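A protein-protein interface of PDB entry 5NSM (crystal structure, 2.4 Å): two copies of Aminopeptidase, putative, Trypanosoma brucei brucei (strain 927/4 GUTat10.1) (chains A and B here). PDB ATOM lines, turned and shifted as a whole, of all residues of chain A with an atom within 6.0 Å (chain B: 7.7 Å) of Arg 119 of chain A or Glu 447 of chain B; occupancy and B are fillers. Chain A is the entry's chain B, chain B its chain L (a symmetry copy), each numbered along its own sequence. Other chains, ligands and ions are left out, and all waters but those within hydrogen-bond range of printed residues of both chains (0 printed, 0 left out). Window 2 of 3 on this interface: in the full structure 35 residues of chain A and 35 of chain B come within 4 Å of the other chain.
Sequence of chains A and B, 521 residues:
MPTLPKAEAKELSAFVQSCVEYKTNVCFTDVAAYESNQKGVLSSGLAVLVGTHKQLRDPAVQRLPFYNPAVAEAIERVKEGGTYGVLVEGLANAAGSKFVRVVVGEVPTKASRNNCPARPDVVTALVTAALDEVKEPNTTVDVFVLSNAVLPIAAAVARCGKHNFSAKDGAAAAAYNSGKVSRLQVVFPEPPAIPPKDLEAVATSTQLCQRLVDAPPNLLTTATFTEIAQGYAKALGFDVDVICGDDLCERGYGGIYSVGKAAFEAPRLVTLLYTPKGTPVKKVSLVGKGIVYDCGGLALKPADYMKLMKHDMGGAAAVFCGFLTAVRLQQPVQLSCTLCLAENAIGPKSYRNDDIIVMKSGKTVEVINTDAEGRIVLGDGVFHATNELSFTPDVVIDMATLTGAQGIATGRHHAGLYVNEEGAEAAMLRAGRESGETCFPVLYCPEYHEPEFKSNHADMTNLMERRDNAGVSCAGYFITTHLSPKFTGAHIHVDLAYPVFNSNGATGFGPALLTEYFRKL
The side-chain amide nitrogen of Asn 115 of chain A lies within hydrogen-bond range of the side-chain carboxylate of Glu 447 of chain B (2.7 Å).
The backbone NH of Ser 112 of chain A lies within hydrogen-bond range of the side-chain carboxylate of Glu 447 of chain B (3.1 Å).
OD1 of Asn 115 of chain A lies within hydrogen-bond range of OH of Tyr 448 of chain B.
The side-chain hydroxyl of Ser 112 of chain A sits at hydrogen-bond distance from the backbone carbonyl oxygen of Tyr 444 of chain B (2.8 Å).
The side-chain hydroxyl (OH) of Tyr 448 of chain B sits close to the side-chain carboxylate (OD1) of Asp 121 of chain A, at 3.4 Å.
The guanidinium group of Arg 119 of chain A lies within hydrogen-bond range of the backbone carbonyl oxygen of Lys 110 of chain A, 2.9 Å away.
A ring nitrogen (NE2) of His 449 of chain B lies within hydrogen-bond range of the backbone NH of Cys 445 of chain B, 3.1 Å away.
The side-chain sulfur (SG) of Cys 445 of chain B sits at hydrogen-bond distance from the side-chain carboxylate (OE2) of Glu 447 of chain B (3.4 Å).
NH1 of Arg 119 of chain A lies within salt-bridge range of OD2 of Asp 121 of chain A (2.9 Å).
Glu 447 of chain B touches Ala 111 of chain A.
OG of Ser 112 of chain A touches CA of Cys 445 of chain B, 3.6 Å away.
Ser 112 of chain A touches Pro 446 of chain B (CB to CD, 3.99 Å).
ND2 of Asn 115 of chain A touches SG of Cys 445 of chain B, 3.9 Å away.
Glu 447 of chain B touches Arg 119 of chain A (CG to NH2, 3.6 Å).
Of the printed residues of chain B, Ala 111 of chain A touches Glu 447 (3.6 Å).
Of the printed residues of chain B, Ser 112 of chain A touches Tyr 444 (2.8 Å), Cys 445 (3.6 Å), Pro 446 (3.99 Å) and Glu 447 (3.1 Å).
No residue of chain B comes within 4 Å of Ala 118 of chain A.
Of the printed residues of chain B, Arg 119 of chain A touches Glu 447 (3.6 Å).
Of the printed residues of chain B, Asp 121 of chain A touches Tyr 448 (3.2 Å).
Val 122 of chain A touches none of the printed residues of chain B.
Of the printed residues of chain A, Pro 446 of chain B touches Ser 112 (3.99 Å).
Glu 447 of chain B touches four residues of chain A.
Of the printed residues of chain A, Tyr 448 of chain B touches Asn 115 (3.4 Å) and Asp 121 (3.2 Å).
The nearest printed residue of chain B that does not touch Asn 115 of chain A is Tyr 444 of chain B (5.8 Å).
Of the 11 printed residues of chain B, 5 touch a printed residue of chain A.
Of the 16 printed residues of chain A, 5 touch a printed residue of chain B.
No position is printed for both chains.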
ATOM      1  N   VAL A 107     -37.027  -1.647  18.146  1.00  0.00           N
ATOM      2  CA  VAL A 107     -36.128  -2.710  17.718  1.00  0.00           C
ATOM      3  C   VAL A 107     -34.692  -2.224  17.866  1.00  0.00           C
ATOM      4  O   VAL A 107     -34.350  -1.163  17.350  1.00  0.00           O
ATOM      5  CB  VAL A 107     -36.355  -3.108  16.229  1.00  0.00           C
ATOM      6  CG1 VAL A 107     -35.486  -4.303  15.836  1.00  0.00           C
ATOM      7  CG2 VAL A 107     -37.828  -3.425  15.948  1.00  0.00           C
ATOM      8  N   PRO A 108     -33.817  -3.015  18.508  1.00  0.00           N
ATOM      9  CA  PRO A 108     -32.415  -2.612  18.554  1.00  0.00           C
ATOM     10  C   PRO A 108     -31.755  -2.582  17.181  1.00  0.00           C
ATOM     11  O   PRO A 108     -32.195  -3.258  16.249  1.00  0.00           O
ATOM     12  CB  PRO A 108     -31.764  -3.681  19.458  1.00  0.00           C
ATOM     13  CG  PRO A 108     -32.698  -4.831  19.461  1.00  0.00           C
ATOM     14  CD  PRO A 108     -34.068  -4.266  19.220  1.00  0.00           C
ATOM     15  N   THR A 109     -30.693  -1.804  17.068  1.00  0.00           N
ATOM     16  CA  THR A 109     -29.830  -1.851  15.857  1.00  0.00           C
ATOM     17  C   THR A 109     -28.625  -2.785  16.058  1.00  0.00           C
ATOM     18  O   THR A 109     -28.049  -3.243  15.085  1.00  0.00           O
ATOM     19  CB  THR A 109     -29.281  -0.486  15.391  1.00  0.00           C
ATOM     20  OG1 THR A 109     -28.787   0.242  16.516  1.00  0.00           O
ATOM     21  CG2 THR A 109     -30.357   0.305  14.672  1.00  0.00           C
ATOM     22  N   LYS A 110     -28.231  -2.985  17.317  1.00  0.00           N
ATOM     23  CA  LYS A 110     -27.127  -3.888  17.682  1.00  0.00           C
ATOM     24  C   LYS A 110     -27.395  -5.247  17.039  1.00  0.00           C
ATOM     25  O   LYS A 110     -28.455  -5.817  17.172  1.00  0.00           O
ATOM     26  CB  LYS A 110     -26.980  -4.028  19.195  1.00  0.00           C
ATOM     27  N   ALA A 111     -26.418  -5.721  16.290  1.00  0.00           N
ATOM     28  CA  ALA A 111     -26.494  -7.017  15.629  1.00  0.00           C
ATOM     29  C   ALA A 111     -25.089  -7.482  15.303  1.00  0.00           C
ATOM     30  O   ALA A 111     -24.360  -6.807  14.600  1.00  0.00           O
ATOM     31  CB  ALA A 111     -27.324  -6.937  14.364  1.00  0.00           C
ATOM     32  N   SER A 112     -24.736  -8.655  15.809  1.00  0.00           N
ATOM     33  CA  SER A 112     -23.394  -9.214  15.622  1.00  0.00           C
ATOM     34  C   SER A 112     -23.305  -9.744  14.201  1.00  0.00           C
ATOM     35  O   SER A 112     -24.310  -9.991  13.565  1.00  0.00           O
ATOM     36  CB  SER A 112     -23.084 -10.345  16.639  1.00  0.00           C
ATOM     37  OG  SER A 112     -23.458 -11.674  16.174  1.00  0.00           O
ATOM     38  N   ASN A 115     -25.628 -12.582  13.181  1.00  0.00           N
ATOM     39  CA  ASN A 115     -27.075 -12.319  13.319  1.00  0.00           C
ATOM     40  C   ASN A 115     -27.668 -11.607  12.090  1.00  0.00           C
ATOM     41  O   ASN A 115     -26.959 -11.110  11.235  1.00  0.00           O
ATOM     42  CB  ASN A 115     -27.344 -11.497  14.582  1.00  0.00           C
ATOM     43  CG  ASN A 115     -28.688 -11.808  15.215  1.00  0.00           C
ATOM     44  OD1 ASN A 115     -29.547 -12.452  14.623  1.00  0.00           O
ATOM     45  ND2 ASN A 115     -28.871 -11.330  16.434  1.00  0.00           N
ATOM     46  N   CYS A 116     -28.988 -11.630  12.025  1.00  0.00           N
ATOM     47  CA  CYS A 116     -29.772 -10.878  11.009  1.00  0.00           C
ATOM     48  C   CYS A 116     -29.842  -9.413  11.436  1.00  0.00           C
ATOM     49  O   CYS A 116     -30.368  -9.135  12.525  1.00  0.00           O
ATOM     50  CB  CYS A 116     -31.190 -11.454  10.863  1.00  0.00           C
ATOM     51  SG  CYS A 116     -32.219 -10.556   9.660  1.00  0.00           S
ATOM     52  N   PRO A 117     -29.268  -8.478  10.640  1.00  0.00           N
ATOM     53  CA  PRO A 117     -29.204  -7.031  11.007  1.00  0.00           C
ATOM     54  C   PRO A 117     -30.545  -6.400  11.373  1.00  0.00           C
ATOM     55  O   PRO A 117     -30.607  -5.488  12.203  1.00  0.00           O
ATOM     56  CB  PRO A 117     -28.693  -6.376   9.732  1.00  0.00           C
ATOM     57  CG  PRO A 117     -27.932  -7.443   9.016  1.00  0.00           C
ATOM     58  CD  PRO A 117     -28.534  -8.758   9.398  1.00  0.00           C
ATOM     59  N   ALA A 118     -31.610  -6.937  10.793  1.00  0.00           N
ATOM     60  CA  ALA A 118     -32.962  -6.423  11.040  1.00  0.00           C
ATOM     61  C   ALA A 118     -33.593  -6.934  12.369  1.00  0.00           C
ATOM     62  O   ALA A 118     -34.686  -6.541  12.736  1.00  0.00           O
ATOM     63  CB  ALA A 118     -33.866  -6.758   9.872  1.00  0.00           C
ATOM     64  N   ARG A 119     -32.891  -7.833  13.043  1.00  0.00           N
ATOM     65  CA  ARG A 119     -33.284  -8.356  14.378  1.00  0.00           C
ATOM     66  C   ARG A 119     -34.752  -8.781  14.436  1.00  0.00           C
ATOM     67  O   ARG A 119     -35.504  -8.313  15.293  1.00  0.00           O
ATOM     68  CB  ARG A 119     -32.962  -7.325  15.460  1.00  0.00           C
ATOM     69  CG  ARG A 119     -31.466  -7.059  15.604  1.00  0.00           C
ATOM     70  CD  ARG A 119     -30.687  -8.266  16.163  1.00  0.00           C
ATOM     71  NE  ARG A 119     -31.267  -8.824  17.381  1.00  0.00           N
ATOM     72  CZ  ARG A 119     -31.031  -8.389  18.612  1.00  0.00           C
ATOM     73  NH1 ARG A 119     -31.662  -8.955  19.631  1.00  0.00           N
ATOM     74  NH2 ARG A 119     -30.185  -7.386  18.833  1.00  0.00           N
ATOM     75  N   PRO A 120     -35.183  -9.658  13.500  1.00  0.00           N
ATOM     76  CA  PRO A 120     -36.549 -10.166  13.505  1.00  0.00           C
ATOM     77  C   PRO A 120     -36.947 -10.914  14.778  1.00  0.00           C
ATOM     78  O   PRO A 120     -38.127 -10.996  15.107  1.00  0.00           O
ATOM     79  CB  PRO A 120     -36.556 -11.122  12.332  1.00  0.00           C
ATOM     80  CG  PRO A 120     -35.164 -11.554  12.203  1.00  0.00           C
ATOM     81  CD  PRO A 120     -34.372 -10.342  12.497  1.00  0.00           C
ATOM     82  N   ASP A 121     -35.963 -11.441  15.490  1.00  0.00           N
ATOM     83  CA  ASP A 121     -36.194 -12.022  16.842  1.00  0.00           C
ATOM     84  C   ASP A 121     -36.943 -11.018  17.777  1.00  0.00           C
ATOM     85  O   ASP A 121     -37.847 -11.398  18.488  1.00  0.00           O
ATOM     86  CB  ASP A 121     -34.888 -12.476  17.518  1.00  0.00           C
ATOM     87  CG  ASP A 121     -33.893 -11.319  17.704  1.00  0.00           C
ATOM     88  OD1 ASP A 121     -33.479 -10.693  16.690  1.00  0.00           O
ATOM     89  OD2 ASP A 121     -33.513 -11.043  18.859  1.00  0.00           O
ATOM     90  N   VAL A 122     -36.535  -9.756  17.746  1.00  0.00           N
ATOM     91  CA  VAL A 122     -37.159  -8.746  18.609  1.00  0.00           C
ATOM     92  C   VAL A 122     -38.491  -8.293  18.021  1.00  0.00           C
ATOM     93  O   VAL A 122     -39.455  -8.088  18.737  1.00  0.00           O
ATOM     94  CB  VAL A 122     -36.264  -7.546  18.888  1.00  0.00           C
ATOM     95  CG1 VAL A 122     -36.996  -6.530  19.778  1.00  0.00           C
ATOM     96  CG2 VAL A 122     -34.993  -7.995  19.573  1.00  0.00           C
ATOM     97  N   VAL A 123     -38.536  -8.205  16.710  1.00  0.00           N
ATOM     98  CA  VAL A 123     -39.810  -7.908  16.011  1.00  0.00           C
ATOM     99  C   VAL A 123     -40.906  -8.881  16.472  1.00  0.00           C
ATOM    100  O   VAL A 123     -42.001  -8.478  16.850  1.00  0.00           O
ATOM    101  CB  VAL A 123     -39.678  -7.953  14.470  1.00  0.00           C
ATOM    102  CG1 VAL A 123     -41.040  -7.839  13.798  1.00  0.00           C
ATOM    103  CG2 VAL A 123     -38.773  -6.822  13.999  1.00  0.00           C
ATOM    104  N   THR A 124     -40.591 -10.160  16.419  1.00  0.00           N
ATOM    105  CA  THR A 124     -41.523 -11.197  16.878  1.00  0.00           C
ATOM    106  C   THR A 124     -42.019 -10.937  18.316  1.00  0.00           C
ATOM    107  O   THR A 124     -43.214 -10.989  18.595  1.00  0.00           O
ATOM    108  CB  THR A 124     -40.897 -12.586  16.806  1.00  0.00           C
ATOM    109  OG1 THR A 124     -40.707 -12.933  15.432  1.00  0.00           O
ATOM    110  CG2 THR A 124     -41.814 -13.675  17.452  1.00  0.00           C
ATOM    111  N   TYR B 418     -13.838 -17.493  20.836  1.00  0.00           N
ATOM    112  CA  TYR B 418     -14.892 -16.499  20.959  1.00  0.00           C
ATOM    113  C   TYR B 418     -14.224 -15.149  20.736  1.00  0.00           C
ATOM    114  O   TYR B 418     -13.423 -14.701  21.535  1.00  0.00           O
ATOM    115  CB  TYR B 418     -15.536 -16.561  22.337  1.00  0.00           C
ATOM    116  CG  TYR B 418     -16.618 -15.489  22.619  1.00  0.00           C
ATOM    117  CD1 TYR B 418     -17.939 -15.702  22.261  1.00  0.00           C
ATOM    118  CD2 TYR B 418     -16.295 -14.303  23.289  1.00  0.00           C
ATOM    119  CE1 TYR B 418     -18.908 -14.769  22.551  1.00  0.00           C
ATOM    120  CE2 TYR B 418     -17.264 -13.348  23.576  1.00  0.00           C
ATOM    121  CZ  TYR B 418     -18.572 -13.594  23.209  1.00  0.00           C
ATOM    122  OH  TYR B 418     -19.528 -12.653  23.424  1.00  0.00           O
ATOM    123  N   TYR B 444     -20.279 -16.059  18.294  1.00  0.00           N
ATOM    124  CA  TYR B 444     -20.182 -14.691  18.839  1.00  0.00           C
ATOM    125  C   TYR B 444     -21.502 -13.951  18.559  1.00  0.00           C
ATOM    126  O   TYR B 444     -21.824 -13.604  17.425  1.00  0.00           O
ATOM    127  CB  TYR B 444     -19.023 -13.894  18.233  1.00  0.00           C
ATOM    128  CG  TYR B 444     -18.857 -12.502  18.831  1.00  0.00           C
ATOM    129  CD1 TYR B 444     -18.204 -12.329  20.042  1.00  0.00           C
ATOM    130  CD2 TYR B 444     -19.389 -11.345  18.196  1.00  0.00           C
ATOM    131  CE1 TYR B 444     -18.066 -11.067  20.612  1.00  0.00           C
ATOM    132  CE2 TYR B 444     -19.237 -10.089  18.754  1.00  0.00           C
ATOM    133  CZ  TYR B 444     -18.577  -9.953  19.957  1.00  0.00           C
ATOM    134  OH  TYR B 444     -18.416  -8.718  20.565  1.00  0.00           O
ATOM    135  N   CYS B 445     -22.252 -13.712  19.617  1.00  0.00           N
ATOM    136  CA  CYS B 445     -23.579 -13.061  19.521  1.00  0.00           C
ATOM    137  C   CYS B 445     -23.996 -12.462  20.882  1.00  0.00           C
ATOM    138  O   CYS B 445     -24.928 -12.953  21.524  1.00  0.00           O
ATOM    139  CB  CYS B 445     -24.634 -14.053  18.999  1.00  0.00           C
ATOM    140  SG  CYS B 445     -26.132 -13.232  18.432  1.00  0.00           S
ATOM    141  N   PRO B 446     -23.296 -11.408  21.321  1.00  0.00           N
ATOM    142  CA  PRO B 446     -23.493 -10.796  22.623  1.00  0.00           C
ATOM    143  C   PRO B 446     -24.946 -10.466  22.977  1.00  0.00           C
ATOM    144  O   PRO B 446     -25.351 -10.600  24.114  1.00  0.00           O
ATOM    145  CB  PRO B 446     -22.695  -9.502  22.532  1.00  0.00           C
ATOM    146  CG  PRO B 446     -21.662  -9.756  21.495  1.00  0.00           C
ATOM    147  CD  PRO B 446     -22.273 -10.707  20.526  1.00  0.00           C
ATOM    148  N   GLU B 447     -25.710 -10.026  21.994  1.00  0.00           N
ATOM    149  CA  GLU B 447     -27.139  -9.732  22.222  1.00  0.00           C
ATOM    150  C   GLU B 447     -27.918 -10.960  22.759  1.00  0.00           C
ATOM    151  O   GLU B 447     -28.917 -10.796  23.437  1.00  0.00           O
ATOM    152  CB  GLU B 447     -27.841  -9.123  20.981  1.00  0.00           C
ATOM    153  CG  GLU B 447     -27.865 -10.012  19.750  1.00  0.00           C
ATOM    154  CD  GLU B 447     -26.667  -9.819  18.804  1.00  0.00           C
ATOM    155  OE1 GLU B 447     -25.538  -9.523  19.273  1.00  0.00           O
ATOM    156  OE2 GLU B 447     -26.857  -9.978  17.584  1.00  0.00           O
ATOM    157  N   TYR B 448     -27.509 -12.152  22.362  1.00  0.00           N
ATOM    158  CA  TYR B 448     -28.157 -13.383  22.857  1.00  0.00           C
ATOM    159  C   TYR B 448     -27.531 -13.959  24.125  1.00  0.00           C
ATOM    160  O   TYR B 448     -28.184 -14.679  24.852  1.00  0.00           O
ATOM    161  CB  TYR B 448     -28.231 -14.479  21.812  1.00  0.00           C
ATOM    162  CG  TYR B 448     -29.102 -14.170  20.603  1.00  0.00           C
ATOM    163  CD1 TYR B 448     -30.062 -13.174  20.638  1.00  0.00           C
ATOM    164  CD2 TYR B 448     -28.984 -14.918  19.445  1.00  0.00           C
ATOM    165  CE1 TYR B 448     -30.874 -12.914  19.539  1.00  0.00           C
ATOM    166  CE2 TYR B 448     -29.762 -14.664  18.343  1.00  0.00           C
ATOM    167  CZ  TYR B 448     -30.711 -13.646  18.389  1.00  0.00           C
ATOM    168  OH  TYR B 448     -31.511 -13.386  17.287  1.00  0.00           O
ATOM    169  N   HIS B 449     -26.301 -13.577  24.417  1.00  0.00           N
ATOM    170  CA  HIS B 449     -25.598 -14.039  25.642  1.00  0.00           C
ATOM    171  C   HIS B 449     -25.954 -13.228  26.848  1.00  0.00           C
ATOM    172  O   HIS B 449     -26.108 -13.745  27.952  1.00  0.00           O
ATOM    173  CB  HIS B 449     -24.080 -13.991  25.487  1.00  0.00           C
ATOM    174  CG  HIS B 449     -23.577 -14.597  24.217  1.00  0.00           C
ATOM    175  ND1 HIS B 449     -24.183 -15.679  23.617  1.00  0.00           N
ATOM    176  CD2 HIS B 449     -22.554 -14.236  23.407  1.00  0.00           C
ATOM    177  CE1 HIS B 449     -23.547 -15.962  22.495  1.00  0.00           C
ATOM    178  NE2 HIS B 449     -22.556 -15.098  22.348  1.00  0.00           N
ATOM    179  N   GLU B 450     -26.079 -11.944  26.619  1.00  0.00           N
ATOM    180  CA  GLU B 450     -26.334 -10.936  27.690  1.00  0.00           C
ATOM    181  C   GLU B 450     -27.526 -11.253  28.655  1.00  0.00           C
ATOM    182  O   GLU B 450     -27.378 -11.099  29.843  1.00  0.00           O
ATOM    183  CB  GLU B 450     -26.463  -9.557  27.050  1.00  0.00           C
ATOM    184  CG  GLU B 450     -26.984  -8.436  27.924  1.00  0.00           C
ATOM    185  CD  GLU B 450     -27.193  -7.132  27.118  1.00  0.00           C
ATOM    186  OE1 GLU B 450     -26.792  -7.057  25.913  1.00  0.00           O
ATOM    187  OE2 GLU B 450     -27.792  -6.183  27.693  1.00  0.00           O
ATOM    188  N   PRO B 451     -28.686 -11.699  28.130  1.00  0.00           N
ATOM    189  CA  PRO B 451     -29.842 -11.956  28.993  1.00  0.00           C
ATOM    190  C   PRO B 451     -29.699 -13.172  29.913  1.00  0.00           C
ATOM    191  O   PRO B 451     -30.412 -13.261  30.904  1.00  0.00           O
ATOM    192  CB  PRO B 451     -30.988 -12.201  28.006  1.00  0.00           C
ATOM    193  CG  PRO B 451     -30.517 -11.661  26.694  1.00  0.00           C
ATOM    194  CD  PRO B 451     -29.037 -11.822  26.701  1.00  0.00           C
ATOM    195  N   GLU B 452     -28.738 -14.039  29.617  1.00  0.00           N
ATOM    196  CA  GLU B 452     -28.490 -15.202  30.464  1.00  0.00           C
ATOM    197  C   GLU B 452     -27.906 -14.856  31.827  1.00  0.00           C
ATOM    198  O   GLU B 452     -27.936 -15.660  32.738  1.00  0.00           O
ATOM    199  CB  GLU B 452     -27.594 -16.216  29.759  1.00  0.00           C
ATOM    200  CG  GLU B 452     -28.266 -16.865  28.544  1.00  0.00           C
ATOM    201  CD  GLU B 452     -29.471 -17.702  28.902  1.00  0.00           C
ATOM    202  OE1 GLU B 452     -29.599 -18.095  30.076  1.00  0.00           O
ATOM    203  OE2 GLU B 452     -30.314 -17.966  28.020  1.00  0.00           O
ATOM    204  N   TYR B 477     -18.526 -14.144  26.838  1.00  0.00           N
ATOM    205  CA  TYR B 477     -19.275 -12.882  26.975  1.00  0.00           C
ATOM    206  C   TYR B 477     -19.042 -12.252  28.353  1.00  0.00           C
ATOM    207  O   TYR B 477     -18.806 -11.059  28.480  1.00  0.00           O
ATOM    208  CB  TYR B 477     -20.766 -13.074  26.737  1.00  0.00           C
ATOM    209  CG  TYR B 477     -21.538 -11.856  27.180  1.00  0.00           C
ATOM    210  CD1 TYR B 477     -21.566 -10.691  26.382  1.00  0.00           C
ATOM    211  CD2 TYR B 477     -22.186 -11.810  28.411  1.00  0.00           C
ATOM    212  CE1 TYR B 477     -22.234  -9.556  26.794  1.00  0.00           C
ATOM    213  CE2 TYR B 477     -22.847 -10.660  28.831  1.00  0.00           C
ATOM    214  CZ  TYR B 477     -22.869  -9.550  28.026  1.00  0.00           C
ATOM    215  OH  TYR B 477     -23.580  -8.427  28.409  1.00  0.00           O
